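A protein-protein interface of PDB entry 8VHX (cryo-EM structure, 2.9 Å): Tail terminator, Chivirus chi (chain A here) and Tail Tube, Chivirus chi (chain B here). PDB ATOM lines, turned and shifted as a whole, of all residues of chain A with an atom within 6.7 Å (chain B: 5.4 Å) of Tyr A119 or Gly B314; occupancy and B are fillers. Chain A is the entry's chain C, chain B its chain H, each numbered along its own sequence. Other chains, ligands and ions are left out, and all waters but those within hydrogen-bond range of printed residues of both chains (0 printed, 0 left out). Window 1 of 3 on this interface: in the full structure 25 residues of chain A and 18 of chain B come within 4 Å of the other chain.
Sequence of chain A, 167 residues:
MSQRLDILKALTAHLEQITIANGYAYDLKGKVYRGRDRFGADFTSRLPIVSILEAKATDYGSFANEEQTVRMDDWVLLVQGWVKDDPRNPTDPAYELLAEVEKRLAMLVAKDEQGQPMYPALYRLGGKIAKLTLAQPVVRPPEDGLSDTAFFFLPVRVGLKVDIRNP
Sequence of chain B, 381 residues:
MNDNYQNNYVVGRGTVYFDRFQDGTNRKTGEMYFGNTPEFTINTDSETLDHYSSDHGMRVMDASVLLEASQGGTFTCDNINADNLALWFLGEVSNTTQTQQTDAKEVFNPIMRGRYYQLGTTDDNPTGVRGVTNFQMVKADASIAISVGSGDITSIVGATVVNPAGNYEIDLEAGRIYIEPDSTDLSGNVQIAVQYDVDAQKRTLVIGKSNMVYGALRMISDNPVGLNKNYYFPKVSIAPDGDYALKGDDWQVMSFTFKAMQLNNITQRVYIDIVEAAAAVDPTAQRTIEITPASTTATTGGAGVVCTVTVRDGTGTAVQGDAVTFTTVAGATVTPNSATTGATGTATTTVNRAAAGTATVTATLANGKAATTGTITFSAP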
ATOM      1  N   LYS A 103       1.448 -24.515  22.465  1.00  0.00           N
ATOM      2  CA  LYS A 103       0.105 -25.070  22.496  1.00  0.00           C
ATOM      3  C   LYS A 103      -0.639 -24.633  23.744  1.00  0.00           C
ATOM      4  O   LYS A 103      -1.845 -24.369  23.699  1.00  0.00           O
ATOM      5  CB  LYS A 103       0.216 -26.585  22.421  1.00  0.00           C
ATOM      6  CG  LYS A 103      -1.040 -27.341  22.184  1.00  0.00           C
ATOM      7  CD  LYS A 103      -0.710 -28.749  21.749  1.00  0.00           C
ATOM      8  CE  LYS A 103       0.180 -29.467  22.753  1.00  0.00           C
ATOM      9  NZ  LYS A 103       0.648 -30.802  22.305  1.00  0.00           N
ATOM     10  N   ALA A 106      -1.377 -20.747  23.416  1.00  0.00           N
ATOM     11  CA  ALA A 106      -2.443 -20.504  22.456  1.00  0.00           C
ATOM     12  C   ALA A 106      -3.815 -20.639  23.085  1.00  0.00           C
ATOM     13  O   ALA A 106      -4.765 -19.989  22.643  1.00  0.00           O
ATOM     14  CB  ALA A 106      -2.321 -21.466  21.293  1.00  0.00           C
ATOM     15  N   MET A 107      -3.939 -21.467  24.114  1.00  0.00           N
ATOM     16  CA  MET A 107      -5.225 -21.657  24.765  1.00  0.00           C
ATOM     17  C   MET A 107      -5.846 -20.336  25.169  1.00  0.00           C
ATOM     18  O   MET A 107      -7.068 -20.245  25.299  1.00  0.00           O
ATOM     19  CB  MET A 107      -5.052 -22.526  26.003  1.00  0.00           C
ATOM     20  CG  MET A 107      -4.317 -23.803  25.775  1.00  0.00           C
ATOM     21  SD  MET A 107      -3.937 -24.614  27.315  1.00  0.00           S
ATOM     22  CE  MET A 107      -5.192 -25.843  27.282  1.00  0.00           C
ATOM     23  N   LEU A 108      -5.022 -19.314  25.362  1.00  0.00           N
ATOM     24  CA  LEU A 108      -5.487 -18.027  25.840  1.00  0.00           C
ATOM     25  C   LEU A 108      -6.168 -17.210  24.762  1.00  0.00           C
ATOM     26  O   LEU A 108      -6.928 -16.295  25.086  1.00  0.00           O
ATOM     27  CB  LEU A 108      -4.309 -17.244  26.389  1.00  0.00           C
ATOM     28  CG  LEU A 108      -3.538 -17.904  27.510  1.00  0.00           C
ATOM     29  CD1 LEU A 108      -2.370 -17.068  27.843  1.00  0.00           C
ATOM     30  CD2 LEU A 108      -4.402 -18.068  28.705  1.00  0.00           C
ATOM     31  N   ALA A 110      -6.864 -18.913  21.498  1.00  0.00           N
ATOM     32  CA  ALA A 110      -7.261 -19.856  20.472  1.00  0.00           C
ATOM     33  C   ALA A 110      -8.772 -19.926  20.386  1.00  0.00           C
ATOM     34  O   ALA A 110      -9.436 -20.426  21.297  1.00  0.00           O
ATOM     35  CB  ALA A 110      -6.678 -21.224  20.765  1.00  0.00           C
ATOM     36  N   GLN A 116     -15.577 -18.863  18.275  1.00  0.00           N
ATOM     37  CA  GLN A 116     -15.793 -18.862  19.704  1.00  0.00           C
ATOM     38  C   GLN A 116     -14.555 -19.363  20.434  1.00  0.00           C
ATOM     39  O   GLN A 116     -13.830 -20.219  19.925  1.00  0.00           O
ATOM     40  CB  GLN A 116     -16.986 -19.733  20.061  1.00  0.00           C
ATOM     41  CG  GLN A 116     -18.230 -19.411  19.287  1.00  0.00           C
ATOM     42  CD  GLN A 116     -18.693 -18.000  19.503  1.00  0.00           C
ATOM     43  OE1 GLN A 116     -18.249 -17.327  20.428  1.00  0.00           O
ATOM     44  NE2 GLN A 116     -19.588 -17.538  18.648  1.00  0.00           N
ATOM     45  N   PRO A 117     -14.291 -18.835  21.622  1.00  0.00           N
ATOM     46  CA  PRO A 117     -13.189 -19.350  22.431  1.00  0.00           C
ATOM     47  C   PRO A 117     -13.282 -20.847  22.657  1.00  0.00           C
ATOM     48  O   PRO A 117     -14.363 -21.398  22.866  1.00  0.00           O
ATOM     49  CB  PRO A 117     -13.338 -18.578  23.736  1.00  0.00           C
ATOM     50  CG  PRO A 117     -14.014 -17.364  23.367  1.00  0.00           C
ATOM     51  CD  PRO A 117     -14.931 -17.684  22.269  1.00  0.00           C
ATOM     52  N   MET A 118     -12.126 -21.509  22.607  1.00  0.00           N
ATOM     53  CA  MET A 118     -12.064 -22.928  22.918  1.00  0.00           C
ATOM     54  C   MET A 118     -12.061 -23.165  24.418  1.00  0.00           C
ATOM     55  O   MET A 118     -12.722 -24.091  24.901  1.00  0.00           O
ATOM     56  CB  MET A 118     -10.820 -23.540  22.288  1.00  0.00           C
ATOM     57  CG  MET A 118     -10.881 -23.683  20.804  1.00  0.00           C
ATOM     58  SD  MET A 118      -9.316 -24.153  20.064  1.00  0.00           S
ATOM     59  CE  MET A 118      -9.187 -25.819  20.670  1.00  0.00           C
ATOM     60  N   TYR A 119     -11.346 -22.332  25.164  1.00  0.00           N
ATOM     61  CA  TYR A 119     -11.201 -22.459  26.612  1.00  0.00           C
ATOM     62  C   TYR A 119     -11.569 -21.115  27.221  1.00  0.00           C
ATOM     63  O   TYR A 119     -10.699 -20.279  27.495  1.00  0.00           O
ATOM     64  CB  TYR A 119      -9.787 -22.882  26.987  1.00  0.00           C
ATOM     65  CG  TYR A 119      -9.320 -24.115  26.286  1.00  0.00           C
ATOM     66  CD1 TYR A 119      -9.708 -25.370  26.704  1.00  0.00           C
ATOM     67  CD2 TYR A 119      -8.489 -24.025  25.197  1.00  0.00           C
ATOM     68  CE1 TYR A 119      -9.279 -26.485  26.054  1.00  0.00           C
ATOM     69  CE2 TYR A 119      -8.055 -25.139  24.547  1.00  0.00           C
ATOM     70  CZ  TYR A 119      -8.450 -26.366  24.977  1.00  0.00           C
ATOM     71  OH  TYR A 119      -8.010 -27.480  24.316  1.00  0.00           O
ATOM     72  N   PRO A 120     -12.860 -20.874  27.440  1.00  0.00           N
ATOM     73  CA  PRO A 120     -13.314 -19.521  27.773  1.00  0.00           C
ATOM     74  C   PRO A 120     -12.789 -18.980  29.084  1.00  0.00           C
ATOM     75  O   PRO A 120     -12.675 -17.758  29.227  1.00  0.00           O
ATOM     76  CB  PRO A 120     -14.831 -19.685  27.815  1.00  0.00           C
ATOM     77  CG  PRO A 120     -15.090 -20.826  26.959  1.00  0.00           C
ATOM     78  CD  PRO A 120     -13.997 -21.771  27.236  1.00  0.00           C
ATOM     79  N   ALA A 121     -12.491 -19.834  30.057  1.00  0.00           N
ATOM     80  CA  ALA A 121     -11.975 -19.342  31.322  1.00  0.00           C
ATOM     81  C   ALA A 121     -10.518 -18.931  31.211  1.00  0.00           C
ATOM     82  O   ALA A 121     -10.088 -17.989  31.883  1.00  0.00           O
ATOM     83  CB  ALA A 121     -12.140 -20.402  32.399  1.00  0.00           C
ATOM     84  N   LEU A 122      -9.755 -19.627  30.376  1.00  0.00           N
ATOM     85  CA  LEU A 122      -8.385 -19.239  30.092  1.00  0.00           C
ATOM     86  C   LEU A 122      -8.319 -18.033  29.180  1.00  0.00           C
ATOM     87  O   LEU A 122      -7.433 -17.188  29.332  1.00  0.00           O
ATOM     88  CB  LEU A 122      -7.667 -20.389  29.414  1.00  0.00           C
ATOM     89  CG  LEU A 122      -7.471 -21.671  30.187  1.00  0.00           C
ATOM     90  CD1 LEU A 122      -6.778 -22.620  29.276  1.00  0.00           C
ATOM     91  CD2 LEU A 122      -6.688 -21.456  31.440  1.00  0.00           C
ATOM     92  N   TYR A 123      -9.250 -17.950  28.242  1.00  0.00           N
ATOM     93  CA  TYR A 123      -9.205 -16.966  27.180  1.00  0.00           C
ATOM     94  C   TYR A 123      -8.804 -15.607  27.719  1.00  0.00           C
ATOM     95  O   TYR A 123      -9.509 -15.009  28.534  1.00  0.00           O
ATOM     96  CB  TYR A 123     -10.573 -16.912  26.516  1.00  0.00           C
ATOM     97  CG  TYR A 123     -10.659 -16.138  25.242  1.00  0.00           C
ATOM     98  CD1 TYR A 123      -9.882 -16.467  24.157  1.00  0.00           C
ATOM     99  CD2 TYR A 123     -11.561 -15.113  25.107  1.00  0.00           C
ATOM    100  CE1 TYR A 123      -9.970 -15.774  22.998  1.00  0.00           C
ATOM    101  CE2 TYR A 123     -11.656 -14.418  23.945  1.00  0.00           C
ATOM    102  CZ  TYR A 123     -10.859 -14.756  22.893  1.00  0.00           C
ATOM    103  OH  TYR A 123     -10.951 -14.059  21.725  1.00  0.00           O
ATOM    104  N   ARG A 124      -7.653 -15.131  27.252  1.00  0.00           N
ATOM    105  CA  ARG A 124      -7.105 -13.841  27.642  1.00  0.00           C
ATOM    106  C   ARG A 124      -6.849 -13.752  29.141  1.00  0.00           C
ATOM    107  O   ARG A 124      -6.856 -12.666  29.717  1.00  0.00           O
ATOM    108  CB  ARG A 124      -8.025 -12.718  27.200  1.00  0.00           C
ATOM    109  CG  ARG A 124      -8.090 -12.521  25.727  1.00  0.00           C
ATOM    110  CD  ARG A 124      -9.129 -11.503  25.399  1.00  0.00           C
ATOM    111  NE  ARG A 124      -9.344 -11.381  23.967  1.00  0.00           N
ATOM    112  CZ  ARG A 124     -10.532 -11.240  23.399  1.00  0.00           C
ATOM    113  NH1 ARG A 124     -10.613 -11.137  22.088  1.00  0.00           N
ATOM    114  NH2 ARG A 124     -11.634 -11.208  24.134  1.00  0.00           N
ATOM    115  N   PRO B 283     -17.190 -23.808  33.427  1.00  0.00           N
ATOM    116  CA  PRO B 283     -16.124 -24.377  32.601  1.00  0.00           C
ATOM    117  C   PRO B 283     -15.883 -25.848  32.851  1.00  0.00           C
ATOM    118  O   PRO B 283     -15.500 -26.562  31.918  1.00  0.00           O
ATOM    119  CB  PRO B 283     -14.906 -23.546  32.999  1.00  0.00           C
ATOM    120  CG  PRO B 283     -15.180 -23.161  34.380  1.00  0.00           C
ATOM    121  CD  PRO B 283     -16.648 -22.906  34.451  1.00  0.00           C
ATOM    122  N   THR B 284     -16.109 -26.331  34.069  1.00  0.00           N
ATOM    123  CA  THR B 284     -15.880 -27.737  34.363  1.00  0.00           C
ATOM    124  C   THR B 284     -16.829 -28.639  33.594  1.00  0.00           C
ATOM    125  O   THR B 284     -16.572 -29.841  33.484  1.00  0.00           O
ATOM    126  CB  THR B 284     -16.025 -27.997  35.862  1.00  0.00           C
ATOM    127  OG1 THR B 284     -17.396 -27.850  36.245  1.00  0.00           O
ATOM    128  CG2 THR B 284     -15.177 -27.022  36.668  1.00  0.00           C
ATOM    129  N   GLN B 286     -17.827 -27.700  30.332  1.00  0.00           N
ATOM    130  CA  GLN B 286     -17.430 -27.587  28.943  1.00  0.00           C
ATOM    131  C   GLN B 286     -16.428 -28.674  28.594  1.00  0.00           C
ATOM    132  O   GLN B 286     -15.823 -29.306  29.462  1.00  0.00           O
ATOM    133  CB  GLN B 286     -16.824 -26.215  28.663  1.00  0.00           C
ATOM    134  CG  GLN B 286     -17.781 -25.082  28.847  1.00  0.00           C
ATOM    135  CD  GLN B 286     -17.386 -23.852  28.078  1.00  0.00           C
ATOM    136  OE1 GLN B 286     -17.024 -23.928  26.906  1.00  0.00           O
ATOM    137  NE2 GLN B 286     -17.466 -22.706  28.728  1.00  0.00           N
ATOM    138  N   ARG B 287     -16.263 -28.894  27.296  1.00  0.00           N
ATOM    139  CA  ARG B 287     -15.386 -29.936  26.804  1.00  0.00           C
ATOM    140  C   ARG B 287     -14.683 -29.458  25.549  1.00  0.00           C
ATOM    141  O   ARG B 287     -15.262 -28.763  24.713  1.00  0.00           O
ATOM    142  CB  ARG B 287     -16.147 -31.225  26.508  1.00  0.00           C
ATOM    143  CG  ARG B 287     -16.635 -31.952  27.734  1.00  0.00           C
ATOM    144  CD  ARG B 287     -15.496 -32.467  28.535  1.00  0.00           C
ATOM    145  NE  ARG B 287     -15.933 -33.257  29.678  1.00  0.00           N
ATOM    146  CZ  ARG B 287     -16.063 -32.782  30.910  1.00  0.00           C
ATOM    147  NH1 ARG B 287     -16.453 -33.584  31.884  1.00  0.00           N
ATOM    148  NH2 ARG B 287     -15.815 -31.513  31.176  1.00  0.00           N
ATOM    149  N   THR B 288     -13.421 -29.844  25.435  1.00  0.00           N
ATOM    150  CA  THR B 288     -12.633 -29.606  24.243  1.00  0.00           C
ATOM    151  C   THR B 288     -11.878 -30.882  23.932  1.00  0.00           C
ATOM    152  O   THR B 288     -11.419 -31.577  24.840  1.00  0.00           O
ATOM    153  CB  THR B 288     -11.660 -28.445  24.422  1.00  0.00           C
ATOM    154  OG1 THR B 288     -12.373 -27.279  24.844  1.00  0.00           O
ATOM    155  CG2 THR B 288     -10.964 -28.156  23.128  1.00  0.00           C
ATOM    156  N   ARG B 312     -10.279 -32.086  27.196  1.00  0.00           N
ATOM    157  CA  ARG B 312     -10.023 -31.044  28.171  1.00  0.00           C
ATOM    158  C   ARG B 312     -11.300 -30.279  28.461  1.00  0.00           C
ATOM    159  O   ARG B 312     -12.192 -30.188  27.617  1.00  0.00           O
ATOM    160  CB  ARG B 312      -8.968 -30.084  27.673  1.00  0.00           C
ATOM    161  CG  ARG B 312      -7.666 -30.710  27.346  1.00  0.00           C
ATOM    162  CD  ARG B 312      -6.670 -29.679  26.956  1.00  0.00           C
ATOM    163  NE  ARG B 312      -5.418 -30.277  26.527  1.00  0.00           N
ATOM    164  CZ  ARG B 312      -4.531 -30.809  27.351  1.00  0.00           C
ATOM    165  NH1 ARG B 312      -3.427 -31.337  26.871  1.00  0.00           N
ATOM    166  NH2 ARG B 312      -4.739 -30.796  28.648  1.00  0.00           N
ATOM    167  N   ASP B 313     -11.378 -29.732  29.665  1.00  0.00           N
ATOM    168  CA  ASP B 313     -12.476 -28.865  30.045  1.00  0.00           C
ATOM    169  C   ASP B 313     -12.150 -27.410  29.715  1.00  0.00           C
ATOM    170  O   ASP B 313     -11.126 -27.093  29.110  1.00  0.00           O
ATOM    171  CB  ASP B 313     -12.806 -29.061  31.524  1.00  0.00           C
ATOM    172  CG  ASP B 313     -11.716 -28.576  32.447  1.00  0.00           C
ATOM    173  OD1 ASP B 313     -10.821 -27.832  32.003  1.00  0.00           O
ATOM    174  OD2 ASP B 313     -11.761 -28.944  33.638  1.00  0.00           O
ATOM    175  N   GLY B 314     -13.037 -26.512  30.125  1.00  0.00           N
ATOM    176  CA  GLY B 314     -12.882 -25.100  29.838  1.00  0.00           C
ATOM    177  C   GLY B 314     -11.701 -24.450  30.514  1.00  0.00           C
ATOM    178  O   GLY B 314     -11.365 -23.312  30.172  1.00  0.00           O
ATOM    179  N   THR B 315     -11.079 -25.128  31.465  1.00  0.00           N
ATOM    180  CA  THR B 315      -9.895 -24.629  32.141  1.00  0.00           C
ATOM    181  C   THR B 315      -8.607 -25.139  31.518  1.00  0.00           C
ATOM    182  O   THR B 315      -7.523 -24.828  32.018  1.00  0.00           O
ATOM    183  CB  THR B 315      -9.926 -25.022  33.615  1.00  0.00           C
ATOM    184  OG1 THR B 315      -9.592 -26.404  33.759  1.00  0.00           O
ATOM    185  CG2 THR B 315     -11.284 -24.809  34.173  1.00  0.00           C
ATOM    186  N   GLY B 316      -8.700 -25.910  30.441  1.00  0.00           N
ATOM    187  CA  GLY B 316      -7.560 -26.594  29.894  1.00  0.00           C
ATOM    188  C   GLY B 316      -7.186 -27.858  30.620  1.00  0.00           C
ATOM    189  O   GLY B 316      -6.260 -28.553  30.187  1.00  0.00           O
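The side-chain hydroxyl (OG1) of Thr B288 sits at hydrogen-bond distance from the backbone carbonyl oxygen (O) of Met A118, at 3.2 Å.
O of Arg B312 lies within hydrogen-bond range of N of Thr B288 (2.5 Å). O of Ala A110 is in hydrogen-bond range of N of Met A118 (3.2 Å). OD1 of Asp B313 is in hydrogen-bond range of N of Gly B316 (3.3 Å). OD1 of Asp B313 is in hydrogen-bond range of OG1 of Thr B315 (2.6 Å). The backbone carbonyl oxygen of Gly B316 lies within hydrogen-bond range of the guanidinium group of Arg B312. O of Pro B283 is in hydrogen-bond range of N of Gly B314.
Among the printed residues, pairs that only touch across the chains: Met A107 with Gly B316, Tyr A119 with Thr B288, Tyr A119 with Arg B312, Tyr A119 with Asp B313, Tyr A119 with Gly B314, Tyr A119 with Gly B316, Pro A120 with Gln B286, Pro A120 with Gly B314, Ala A121 with Gly B314, Leu A122 with Thr B315 and Leu A122 with Gly B316.
Of the printed residues of chain B, Met A107 touches Gly B316 (3.6 Å). Of the printed residues of chain B, Met A118 touches Thr B288. Tyr A119 touches five residues of chain B. Of the printed residues of chain B, Ala A121 touches Gly B314 (3.7 Å). Of chain A, only Tyr A119, Pro A120 and Ala A121 come within 4 Å of Gly B314. Printed residues of chain A within 4 Å of Gly B316: Met A107 (3.6 Å), Tyr A119 (3.9 Å) and Leu A122 (3.98 Å). The nearest residue of chain B that does not touch Tyr A119 is Thr B315 (4.9 Å).
Hydrophobic or aromatic side chains of chain A within 4 Å of the printed part of chain B: Met A107, Met A118, Tyr A119, Pro A120, Ala A121 and Leu A122. Among the printed residues, 12 pairs touch across the chains.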
